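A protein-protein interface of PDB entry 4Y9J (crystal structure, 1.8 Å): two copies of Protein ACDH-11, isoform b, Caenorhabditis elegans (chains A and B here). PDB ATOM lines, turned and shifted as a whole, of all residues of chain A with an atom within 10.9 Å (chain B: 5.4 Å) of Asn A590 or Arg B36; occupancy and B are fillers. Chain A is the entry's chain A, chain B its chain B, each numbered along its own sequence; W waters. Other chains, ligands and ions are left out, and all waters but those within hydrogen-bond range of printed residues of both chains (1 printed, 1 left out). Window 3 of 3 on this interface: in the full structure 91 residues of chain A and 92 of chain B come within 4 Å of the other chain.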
ATOM      1  N   ASP A 583      31.034 -23.705  17.366  1.00  0.00           N
ATOM      2  CA  ASP A 583      30.438 -24.938  16.843  1.00  0.00           C
ATOM      3  C   ASP A 583      28.978 -24.695  16.536  1.00  0.00           C
ATOM      4  O   ASP A 583      28.475 -25.160  15.528  1.00  0.00           O
ATOM      5  CB  ASP A 583      30.500 -26.115  17.849  1.00  0.00           C
ATOM      6  CG  ASP A 583      31.934 -26.535  18.232  1.00  0.00           C
ATOM      7  OD1 ASP A 583      32.909 -26.310  17.448  1.00  0.00           O
ATOM      8  OD2 ASP A 583      32.056 -27.124  19.348  1.00  0.00           O
ATOM      9  N   ARG A 584      28.270 -23.998  17.414  1.00  0.00           N
ATOM     10  CA  ARG A 584      26.848 -23.774  17.195  1.00  0.00           C
ATOM     11  C   ARG A 584      26.564 -22.903  15.947  1.00  0.00           C
ATOM     12  O   ARG A 584      25.597 -23.122  15.209  1.00  0.00           O
ATOM     13  CB  ARG A 584      26.227 -23.126  18.413  1.00  0.00           C
ATOM     14  CG  ARG A 584      26.011 -24.090  19.570  1.00  0.00           C
ATOM     15  CD  ARG A 584      25.720 -23.320  20.861  1.00  0.00           C
ATOM     16  NE  ARG A 584      25.526 -24.296  21.912  1.00  0.00           N
ATOM     17  CZ  ARG A 584      25.564 -24.039  23.210  1.00  0.00           C
ATOM     18  NH1 ARG A 584      25.787 -22.814  23.656  1.00  0.00           N
ATOM     19  NH2 ARG A 584      25.345 -25.035  24.060  1.00  0.00           N
ATOM     20  N   GLU A 585      27.433 -21.967  15.685  1.00  0.00           N
ATOM     21  CA  GLU A 585      27.279 -21.126  14.543  1.00  0.00           C
ATOM     22  C   GLU A 585      27.537 -21.838  13.251  1.00  0.00           C
ATOM     23  O   GLU A 585      26.915 -21.517  12.239  1.00  0.00           O
ATOM     24  CB  GLU A 585      28.188 -19.902  14.641  1.00  0.00           C
ATOM     25  CG  GLU A 585      27.694 -18.956  15.706  1.00  0.00           C
ATOM     26  CD  GLU A 585      28.443 -17.644  15.724  1.00  0.00           C
ATOM     27  OE1 GLU A 585      29.234 -17.350  14.784  1.00  0.00           O
ATOM     28  OE2 GLU A 585      28.209 -16.895  16.694  1.00  0.00           O
ATOM     29  N   ILE A 586      28.497 -22.737  13.262  1.00  0.00           N
ATOM     30  CA  ILE A 586      28.717 -23.676  12.154  1.00  0.00           C
ATOM     31  C   ILE A 586      27.503 -24.544  11.879  1.00  0.00           C
ATOM     32  O   ILE A 586      27.034 -24.567  10.755  1.00  0.00           O
ATOM     33  CB  ILE A 586      30.009 -24.502  12.361  1.00  0.00           C
ATOM     34  CG1 ILE A 586      31.252 -23.609  12.233  1.00  0.00           C
ATOM     35  CG2 ILE A 586      30.140 -25.635  11.357  1.00  0.00           C
ATOM     36  CD1 ILE A 586      32.537 -24.265  12.784  1.00  0.00           C
ATOM     37  N   VAL A 587      26.991 -25.248  12.874  1.00  0.00           N
ATOM     38  CA  VAL A 587      25.912 -26.184  12.716  1.00  0.00           C
ATOM     39  C   VAL A 587      24.575 -25.552  12.252  1.00  0.00           C
ATOM     40  O   VAL A 587      23.916 -26.051  11.350  1.00  0.00           O
ATOM     41  CB  VAL A 587      25.724 -26.963  14.041  1.00  0.00           C
ATOM     42  CG1 VAL A 587      24.537 -27.927  13.973  1.00  0.00           C
ATOM     43  CG2 VAL A 587      26.989 -27.743  14.328  1.00  0.00           C
ATOM     44  N   PHE A 588      24.228 -24.444  12.873  1.00  0.00           N
ATOM     45  CA  PHE A 588      22.930 -23.825  12.685  1.00  0.00           C
ATOM     46  C   PHE A 588      22.882 -22.680  11.685  1.00  0.00           C
ATOM     47  O   PHE A 588      21.864 -21.975  11.582  1.00  0.00           O
ATOM     48  CB  PHE A 588      22.389 -23.461  14.049  1.00  0.00           C
ATOM     49  CG  PHE A 588      22.048 -24.673  14.855  1.00  0.00           C
ATOM     50  CD1 PHE A 588      20.919 -25.399  14.549  1.00  0.00           C
ATOM     51  CD2 PHE A 588      22.894 -25.143  15.858  1.00  0.00           C
ATOM     52  CE1 PHE A 588      20.602 -26.534  15.240  1.00  0.00           C
ATOM     53  CE2 PHE A 588      22.574 -26.259  16.557  1.00  0.00           C
ATOM     54  CZ  PHE A 588      21.430 -26.986  16.250  1.00  0.00           C
ATOM     55  N   ASP A 589      23.958 -22.475  10.939  1.00  0.00           N
ATOM     56  CA  ASP A 589      23.993 -21.451   9.866  1.00  0.00           C
ATOM     57  C   ASP A 589      22.840 -21.640   8.860  1.00  0.00           C
ATOM     58  O   ASP A 589      22.705 -22.698   8.224  1.00  0.00           O
ATOM     59  CB  ASP A 589      25.313 -21.608   9.141  1.00  0.00           C
ATOM     60  CG  ASP A 589      25.636 -20.477   8.205  1.00  0.00           C
ATOM     61  OD1 ASP A 589      24.900 -19.462   8.138  1.00  0.00           O
ATOM     62  OD2 ASP A 589      26.697 -20.607   7.568  1.00  0.00           O
ATOM     63  N   ASN A 590      21.994 -20.627   8.761  1.00  0.00           N
ATOM     64  CA  ASN A 590      20.831 -20.599   7.869  1.00  0.00           C
ATOM     65  C   ASN A 590      19.753 -21.567   8.312  1.00  0.00           C
ATOM     66  O   ASN A 590      18.891 -21.907   7.499  1.00  0.00           O
ATOM     67  CB  ASN A 590      21.216 -20.938   6.427  1.00  0.00           C
ATOM     68  CG  ASN A 590      21.675 -19.747   5.665  1.00  0.00           C
ATOM     69  OD1 ASN A 590      21.236 -18.652   5.937  1.00  0.00           O
ATOM     70  ND2 ASN A 590      22.530 -19.947   4.682  1.00  0.00           N
ATOM     71  N   PHE A 591      19.773 -21.995   9.581  1.00  0.00           N
ATOM     72  CA  PHE A 591      18.726 -22.894  10.104  1.00  0.00           C
ATOM     73  C   PHE A 591      17.320 -22.262  10.100  1.00  0.00           C
ATOM     74  O   PHE A 591      17.134 -21.148  10.572  1.00  0.00           O
ATOM     75  CB  PHE A 591      19.021 -23.420  11.530  1.00  0.00           C
ATOM     76  CG  PHE A 591      17.927 -24.339  12.056  1.00  0.00           C
ATOM     77  CD1 PHE A 591      17.596 -25.492  11.372  1.00  0.00           C
ATOM     78  CD2 PHE A 591      17.184 -23.991  13.181  1.00  0.00           C
ATOM     79  CE1 PHE A 591      16.599 -26.340  11.831  1.00  0.00           C
ATOM     80  CE2 PHE A 591      16.189 -24.824  13.662  1.00  0.00           C
ATOM     81  CZ  PHE A 591      15.889 -26.017  12.993  1.00  0.00           C
ATOM     82  N   THR A 592      16.307 -23.008   9.619  1.00  0.00           N
ATOM     83  CA  THR A 592      14.936 -22.465   9.650  1.00  0.00           C
ATOM     84  C   THR A 592      14.013 -23.192  10.652  1.00  0.00           C
ATOM     85  O   THR A 592      13.752 -22.608  11.713  1.00  0.00           O
ATOM     86  CB  THR A 592      14.360 -22.288   8.203  1.00  0.00           C
ATOM     87  OG1 THR A 592      14.570 -23.476   7.403  1.00  0.00           O
ATOM     88  CG2 THR A 592      15.095 -21.064   7.510  1.00  0.00           C
ATOM     89  N   LYS B  29      16.954 -22.638   0.654  1.00  0.00           N
ATOM     90  CA  LYS B  29      16.976 -21.631   1.714  1.00  0.00           C
ATOM     91  C   LYS B  29      17.732 -22.078   2.961  1.00  0.00           C
ATOM     92  O   LYS B  29      18.345 -21.296   3.615  1.00  0.00           O
ATOM     93  CB  LYS B  29      15.570 -21.281   2.135  1.00  0.00           C
ATOM     94  CG  LYS B  29      14.824 -20.481   1.077  1.00  0.00           C
ATOM     95  CD  LYS B  29      13.363 -20.271   1.446  1.00  0.00           C
ATOM     96  CE  LYS B  29      12.656 -19.578   0.321  1.00  0.00           C
ATOM     97  NZ  LYS B  29      11.239 -19.337   0.663  1.00  0.00           N
ATOM     98  N   ASP B  30      17.638 -23.367   3.274  1.00  0.00           N
ATOM     99  CA  ASP B  30      18.130 -23.910   4.507  1.00  0.00           C
ATOM    100  C   ASP B  30      19.578 -24.272   4.369  1.00  0.00           C
ATOM    101  O   ASP B  30      20.220 -24.537   5.419  1.00  0.00           O
ATOM    102  CB  ASP B  30      17.301 -25.157   4.878  1.00  0.00           C
ATOM    103  CG  ASP B  30      17.515 -25.630   6.352  1.00  0.00           C
ATOM    104  OD1 ASP B  30      17.111 -24.895   7.310  1.00  0.00           O
ATOM    105  OD2 ASP B  30      18.059 -26.740   6.519  1.00  0.00           O
ATOM    106  N   ASP B  31      20.113 -24.334   3.138  1.00  0.00           N
ATOM    107  CA  ASP B  31      21.506 -24.791   2.977  1.00  0.00           C
ATOM    108  C   ASP B  31      22.459 -23.723   3.580  1.00  0.00           C
ATOM    109  O   ASP B  31      22.322 -22.542   3.256  1.00  0.00           O
ATOM    110  CB  ASP B  31      21.899 -25.068   1.518  1.00  0.00           C
ATOM    111  CG  ASP B  31      23.226 -25.860   1.382  1.00  0.00           C
ATOM    112  OD1 ASP B  31      24.322 -25.246   1.334  1.00  0.00           O
ATOM    113  OD2 ASP B  31      23.175 -27.110   1.266  1.00  0.00           O
ATOM    114  N   PRO B  32      23.430 -24.165   4.404  1.00  0.00           N
ATOM    115  CA  PRO B  32      24.457 -23.294   4.972  1.00  0.00           C
ATOM    116  C   PRO B  32      25.252 -22.479   3.979  1.00  0.00           C
ATOM    117  O   PRO B  32      25.512 -21.325   4.251  1.00  0.00           O
ATOM    118  CB  PRO B  32      25.368 -24.291   5.671  1.00  0.00           C
ATOM    119  CG  PRO B  32      24.441 -25.346   6.161  1.00  0.00           C
ATOM    120  CD  PRO B  32      23.481 -25.504   5.021  1.00  0.00           C
ATOM    121  N   ILE B  33      25.670 -23.046   2.856  1.00  0.00           N
ATOM    122  CA  ILE B  33      26.555 -22.333   1.953  1.00  0.00           C
ATOM    123  C   ILE B  33      26.208 -22.229   0.484  1.00  0.00           C
ATOM    124  O   ILE B  33      26.866 -21.484  -0.216  1.00  0.00           O
ATOM    125  CB  ILE B  33      27.988 -22.887   1.914  1.00  0.00           C
ATOM    126  CG1 ILE B  33      28.024 -24.314   1.464  1.00  0.00           C
ATOM    127  CG2 ILE B  33      28.756 -22.662   3.213  1.00  0.00           C
ATOM    128  CD1 ILE B  33      29.420 -24.653   1.000  1.00  0.00           C
ATOM    129  N   LEU B  34      25.212 -22.964   0.004  1.00  0.00           N
ATOM    130  CA  LEU B  34      24.822 -22.907  -1.402  1.00  0.00           C
ATOM    131  C   LEU B  34      24.536 -21.516  -1.969  1.00  0.00           C
ATOM    132  O   LEU B  34      25.057 -21.161  -3.023  1.00  0.00           O
ATOM    133  CB  LEU B  34      23.575 -23.780  -1.620  1.00  0.00           C
ATOM    134  CG  LEU B  34      23.186 -23.914  -3.074  1.00  0.00           C
ATOM    135  CD1 LEU B  34      24.375 -24.330  -3.923  1.00  0.00           C
ATOM    136  CD2 LEU B  34      22.058 -24.925  -3.099  1.00  0.00           C
ATOM    137  N   ASP B  35      23.659 -20.768  -1.311  1.00  0.00           N
ATOM    138  CA  ASP B  35      23.308 -19.458  -1.806  1.00  0.00           C
ATOM    139  C   ASP B  35      24.538 -18.512  -1.759  1.00  0.00           C
ATOM    140  O   ASP B  35      24.773 -17.772  -2.718  1.00  0.00           O
ATOM    141  CB  ASP B  35      22.145 -18.880  -0.992  1.00  0.00           C
ATOM    142  CG  ASP B  35      21.700 -17.462  -1.469  1.00  0.00           C
ATOM    143  OD1 ASP B  35      21.060 -17.348  -2.551  1.00  0.00           O
ATOM    144  OD2 ASP B  35      21.967 -16.483  -0.740  1.00  0.00           O
ATOM    145  N   ARG B  36      25.296 -18.499  -0.653  1.00  0.00           N
ATOM    146  CA  ARG B  36      26.517 -17.668  -0.558  1.00  0.00           C
ATOM    147  C   ARG B  36      27.494 -17.991  -1.687  1.00  0.00           C
ATOM    148  O   ARG B  36      28.080 -17.091  -2.243  1.00  0.00           O
ATOM    149  CB  ARG B  36      27.201 -17.772   0.813  1.00  0.00           C
ATOM    150  CG  ARG B  36      26.456 -17.067   1.939  1.00  0.00           C
ATOM    151  CD  ARG B  36      27.326 -16.699   3.126  1.00  0.00           C
ATOM    152  NE  ARG B  36      28.046 -17.793   3.806  1.00  0.00           N
ATOM    153  CZ  ARG B  36      27.491 -18.721   4.589  1.00  0.00           C
ATOM    154  NH1 ARG B  36      26.180 -18.745   4.812  1.00  0.00           N
ATOM    155  NH2 ARG B  36      28.258 -19.653   5.162  1.00  0.00           N
ATOM    156  N   THR B  37      27.616 -19.266  -2.047  1.00  0.00           N
ATOM    157  CA  THR B  37      28.537 -19.746  -3.068  1.00  0.00           C
ATOM    158  C   THR B  37      28.100 -19.316  -4.448  1.00  0.00           C
ATOM    159  O   THR B  37      28.936 -18.862  -5.244  1.00  0.00           O
ATOM    160  CB  THR B  37      28.613 -21.271  -3.033  1.00  0.00           C
ATOM    161  OG1 THR B  37      29.014 -21.668  -1.731  1.00  0.00           O
ATOM    162  CG2 THR B  37      29.584 -21.811  -4.081  1.00  0.00           C
ATOM    163  N   LEU B  38      26.794 -19.405  -4.731  1.00  0.00           N
ATOM    164  CA  LEU B  38      26.256 -18.924  -6.009  1.00  0.00           C
ATOM    165  C   LEU B  38      26.412 -17.400  -6.192  1.00  0.00           C
ATOM    166  O   LEU B  38      26.711 -16.891  -7.289  1.00  0.00           O
ATOM    167  CB  LEU B  38      24.761 -19.305  -6.186  1.00  0.00           C
ATOM    168  CG  LEU B  38      24.444 -20.801  -6.151  1.00  0.00           C
ATOM    169  CD1 LEU B  38      22.939 -21.032  -6.366  1.00  0.00           C
ATOM    170  CD2 LEU B  38      25.346 -21.563  -7.119  1.00  0.00           C
ATOM    171  N   ARG B  39      26.161 -16.662  -5.126  1.00  0.00           N
ATOM    172  CA  ARG B  39      26.444 -15.220  -5.132  1.00  0.00           C
ATOM    173  C   ARG B  39      27.873 -14.873  -5.569  1.00  0.00           C
ATOM    174  O   ARG B  39      28.069 -13.888  -6.220  1.00  0.00           O
ATOM    175  CB  ARG B  39      26.244 -14.630  -3.751  1.00  0.00           C
ATOM    176  CG  ARG B  39      24.822 -14.369  -3.345  1.00  0.00           C
ATOM    177  CD  ARG B  39      24.776 -13.831  -1.925  1.00  0.00           C
ATOM    178  NE  ARG B  39      23.386 -13.639  -1.561  1.00  0.00           N
ATOM    179  CZ  ARG B  39      22.659 -12.589  -1.937  1.00  0.00           C
ATOM    180  NH1 ARG B  39      23.198 -11.603  -2.659  1.00  0.00           N
ATOM    181  NH2 ARG B  39      21.384 -12.511  -1.576  1.00  0.00           N
ATOM    182  N   ARG B  40      28.863 -15.665  -5.174  1.00  0.00           N
ATOM    183  CA  ARG B  40      30.256 -15.409  -5.523  1.00  0.00           C
ATOM    184  C   ARG B  40      30.588 -15.797  -6.921  1.00  0.00           C
ATOM    185  O   ARG B  40      31.369 -15.149  -7.559  1.00  0.00           O
ATOM    186  CB  ARG B  40      31.182 -16.234  -4.649  1.00  0.00           C
ATOM    187  CG  ARG B  40      31.102 -15.839  -3.212  1.00  0.00           C
ATOM    188  CD  ARG B  40      32.157 -16.581  -2.396  1.00  0.00           C
ATOM    189  NE  ARG B  40      33.475 -16.096  -2.810  1.00  0.00           N
ATOM    190  CZ  ARG B  40      34.424 -16.828  -3.390  1.00  0.00           C
ATOM    191  NH1 ARG B  40      34.252 -18.160  -3.609  1.00  0.00           N
ATOM    192  NH2 ARG B  40      35.563 -16.203  -3.723  1.00  0.00           N
ATOM    193  N   ARG B 335      20.311 -31.829  12.402  1.00  0.00           N
ATOM    194  CA  ARG B 335      20.238 -30.597  13.122  1.00  0.00           C
ATOM    195  C   ARG B 335      18.822 -30.116  13.503  1.00  0.00           C
ATOM    196  O   ARG B 335      18.628 -29.602  14.615  1.00  0.00           O
ATOM    197  CB  ARG B 335      21.045 -29.434  12.501  1.00  0.00           C
ATOM    198  CG  ARG B 335      20.374 -28.744  11.366  1.00  0.00           C
ATOM    199  CD  ARG B 335      21.287 -27.682  10.743  1.00  0.00           C
ATOM    200  NE  ARG B 335      20.562 -26.987   9.684  1.00  0.00           N
ATOM    201  CZ  ARG B 335      20.970 -25.871   9.094  1.00  0.00           C
ATOM    202  NH1 ARG B 335      22.088 -25.279   9.454  1.00  0.00           N
ATOM    203  NH2 ARG B 335      20.209 -25.323   8.153  1.00  0.00           N
ATOM    204  N   ARG B 366      31.381 -28.859   3.771  1.00  0.00           N
ATOM    205  CA  ARG B 366      31.569 -27.599   3.089  1.00  0.00           C
ATOM    206  C   ARG B 366      32.761 -27.649   2.149  1.00  0.00           C
ATOM    207  O   ARG B 366      32.703 -27.097   1.054  1.00  0.00           O
ATOM    208  CB  ARG B 366      31.719 -26.457   4.062  1.00  0.00           C
ATOM    209  CG  ARG B 366      30.460 -26.150   4.806  1.00  0.00           C
ATOM    210  CD  ARG B 366      30.580 -24.877   5.598  1.00  0.00           C
ATOM    211  NE  ARG B 366      29.456 -24.612   6.477  1.00  0.00           N
ATOM    212  CZ  ARG B 366      29.229 -23.419   7.024  1.00  0.00           C
ATOM    213  NH1 ARG B 366      30.041 -22.368   6.807  1.00  0.00           N
ATOM    214  NH2 ARG B 366      28.181 -23.282   7.814  1.00  0.00           N
ATOM    215  N   HIS B 543      36.858 -18.609  -0.343  1.00  0.00           N
ATOM    216  CA  HIS B 543      35.497 -18.322   0.068  1.00  0.00           C
ATOM    217  C   HIS B 543      35.373 -17.475   1.333  1.00  0.00           C
ATOM    218  O   HIS B 543      34.609 -16.504   1.345  1.00  0.00           O
ATOM    219  CB  HIS B 543      34.779 -19.629   0.264  1.00  0.00           C
ATOM    220  CG  HIS B 543      33.332 -19.492   0.608  1.00  0.00           C
ATOM    221  ND1 HIS B 543      32.860 -19.554   1.903  1.00  0.00           N
ATOM    222  CD2 HIS B 543      32.244 -19.382  -0.182  1.00  0.00           C
ATOM    223  CE1 HIS B 543      31.542 -19.466   1.893  1.00  0.00           C
ATOM    224  NE2 HIS B 543      31.150 -19.333   0.640  1.00  0.00           N
ATOM    225  N   VAL B 549      30.672 -11.665   1.084  1.00  0.00           N
ATOM    226  CA  VAL B 549      29.646 -12.670   1.371  1.00  0.00           C
ATOM    227  C   VAL B 549      29.977 -13.524   2.599  1.00  0.00           C
ATOM    228  O   VAL B 549      29.065 -13.996   3.265  1.00  0.00           O
ATOM    229  CB  VAL B 549      29.294 -13.601   0.153  1.00  0.00           C
ATOM    230  CG1 VAL B 549      29.315 -12.829  -1.166  1.00  0.00           C
ATOM    231  CG2 VAL B 549      30.224 -14.791   0.060  1.00  0.00           C
ATOM    232  N   ALA B 550      31.255 -13.681   2.910  1.00  0.00           N
ATOM    233  CA  ALA B 550      31.673 -14.598   3.972  1.00  0.00           C
ATOM    234  C   ALA B 550      31.067 -14.178   5.299  1.00  0.00           C
ATOM    235  O   ALA B 550      30.943 -12.978   5.546  1.00  0.00           O
ATOM    236  CB  ALA B 550      33.191 -14.577   4.080  1.00  0.00           C
ATOM    237  N   ASN B 551      30.669 -15.131   6.150  1.00  0.00           N
ATOM    238  CA  ASN B 551      30.411 -14.806   7.564  1.00  0.00           C
ATOM    239  C   ASN B 551      31.477 -15.465   8.457  1.00  0.00           C
ATOM    240  O   ASN B 551      32.354 -16.177   7.969  1.00  0.00           O
ATOM    241  CB  ASN B 551      28.992 -15.216   7.971  1.00  0.00           C
ATOM    242  CG  ASN B 551      28.752 -16.694   7.812  1.00  0.00           C
ATOM    243  OD1 ASN B 551      29.656 -17.499   8.026  1.00  0.00           O
ATOM    244  ND2 ASN B 551      27.560 -17.061   7.378  1.00  0.00           N
ATOM    245  N   SER B 553      31.395 -17.995  10.403  1.00  0.00           N
ATOM    246  CA  SER B 553      31.439 -19.467  10.293  1.00  0.00           C
ATOM    247  C   SER B 553      32.341 -19.844   9.108  1.00  0.00           C
ATOM    248  O   SER B 553      33.052 -20.845   9.160  1.00  0.00           O
ATOM    249  CB  SER B 553      30.045 -20.062  10.101  1.00  0.00           C
ATOM    250  OG  SER B 553      29.642 -20.187   8.701  1.00  0.00           O
ATOM    251  N   ASP B 554      32.376 -19.020   8.057  1.00  0.00           N
ATOM    252  CA  ASP B 554      33.164 -19.360   6.893  1.00  0.00           C
ATOM    253  C   ASP B 554      34.646 -19.359   7.236  1.00  0.00           C
ATOM    254  O   ASP B 554      35.392 -20.236   6.772  1.00  0.00           O
ATOM    255  CB  ASP B 554      32.886 -18.393   5.723  1.00  0.00           C
ATOM    256  CG  ASP B 554      31.491 -18.601   5.089  1.00  0.00           C
ATOM    257  OD1 ASP B 554      31.015 -19.756   4.944  1.00  0.00           O
ATOM    258  OD2 ASP B 554      30.860 -17.587   4.673  1.00  0.00           O
HETATM  259  O   HOH W   1      24.401 -27.563   8.954  1.00  0.00           O
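The guanidinium group (NH1) of Arg B36 lies close to the side-chain amide nitrogen (ND2) of Asn B551 (3.4 Å). The guanidinium group of Arg B366 lies within salt-bridge range of the side-chain carboxylate of Asp B554. The side-chain carboxylate (OD2) of Asp B554 lies within hydrogen-bond range of the backbone NH (N) of Asn B551 (2.9 Å). OD1 of Asp B31 is in hydrogen-bond range of N of Leu B34 (2.8 Å). OD1 of Asp B554 is in salt-bridge range of NH2 of Arg B36 (2.8 Å). The backbone carbonyl oxygen of Pro B32 lies within hydrogen-bond range of the guanidinium group of Arg B36, at 2.7 Å.
Among the printed residues, 18 pairs touch across the chains. Among the printed residues, Asp or Glu carboxylates within 4 Å of a Lys or Arg side-chain nitrogen of the other chain: Asp A589 with Arg B36 and Asp A589 with Arg B366.
O of Asn A590 sits close to OD1 of Asp B30 (3.5 Å). The backbone carbonyl oxygen (O) of Val A587 is in hydrogen-bond range of the guanidinium group (NH1) of Arg B335 (2.7 Å). OD1 of Asp B30 sits at hydrogen-bond distance from OG1 of Thr A592 (2.9 Å). ND2 of Asn A590 sits at hydrogen-bond distance from O of Pro B32 (3.3 Å). The guanidinium group (NH2) of Arg B366 lies within hydrogen-bond range of the backbone carbonyl oxygen (O) of Ile A586 (3.4 Å). The guanidinium group (NH2) of Arg B366 is in salt-bridge range of the side-chain carboxylate (OD2) of Asp A589. O of Asp A589 is in hydrogen-bond range of NH1 of Arg B335. ND2 of Asn A590 lies within hydrogen-bond range of O of Asp B31, at 3.0 Å. The side-chain hydroxyl (OG) of Ser B553 sits at hydrogen-bond distance from the side-chain carboxylate (OD2) of Asp A589 (3.2 Å). OD2 of Asp A589 is in salt-bridge range of NH2 of Arg B36 (3.0 Å).
Arg B335 touches Phe A588 (NH1 to C, 3.5 Å). O of Pro B32 touches OD2 of Asp A589, 3.6 Å away. Asp A589 touches Asn B551. Asn A590 touches Lys B29. Arg B36 touches Asn A590. Arg B335 touches Asn A590. OD1 of Asp B30 touches CA of Phe A591 (3.8 Å). Phe A591 touches Arg B335 (CA to NH2, 3.5 Å).
Water W1 bridges the backbone carbonyl oxygen (O) of Val A587 (2.9 Å) and the guanidinium group (NH1) of Arg B335 (3.3 Å).
Printed residues of chain B within 4 Å of Ile A586: Arg B366 (3.4 Å). Of the printed residues of chain B, Val A587 touches Arg B335. Printed residues of chain B within 4 Å of Asp A589: Pro B32 (3.6 Å), Arg B36 (3.0 Å), Arg B335 (2.9 Å), Arg B366 (3.1 Å), Asn B551 (3.7 Å) and Ser B553 (3.2 Å). Of chain B, only Lys B29 (3.97 Å), Asp B30 (3.5 Å), Asp B31 (3.0 Å), Pro B32 (3.3 Å), Arg B36 (3.8 Å) and Arg B335 (3.7 Å) come within 4 Å of Asn A590. Of the printed residues of chain B, Thr A592 touches Asp B30 (2.9 Å). Printed residues of chain A within 4 Å of Asp B31: Asn A590 (3.0 Å). Of the printed residues of chain A, Pro B32 touches Asp A589 and Asn A590. Ile B33 touches none of the printed residues of chain A. Arg B36 touches just these residues of chain A: Asp A589 (3.0 Å) and Asn A590 (3.8 Å). Arg B39 touches none of the printed residues of chain A. Arg B40 touches none of the printed residues of chain A. No residue of chain A comes within 4 Å of Val B549. No residue of chain A comes within 4 Å of Ala B550. Of chain A, only Asp A589 (3.7 Å) comes within 4 Å of Asn B551. Ser B553 touches just one residue of chain A: Asp A589 (3.2 Å). The nearest residue of chain A that does not touch Arg B36 is Glu A585 (7.4 Å).
No position is printed for both chains.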
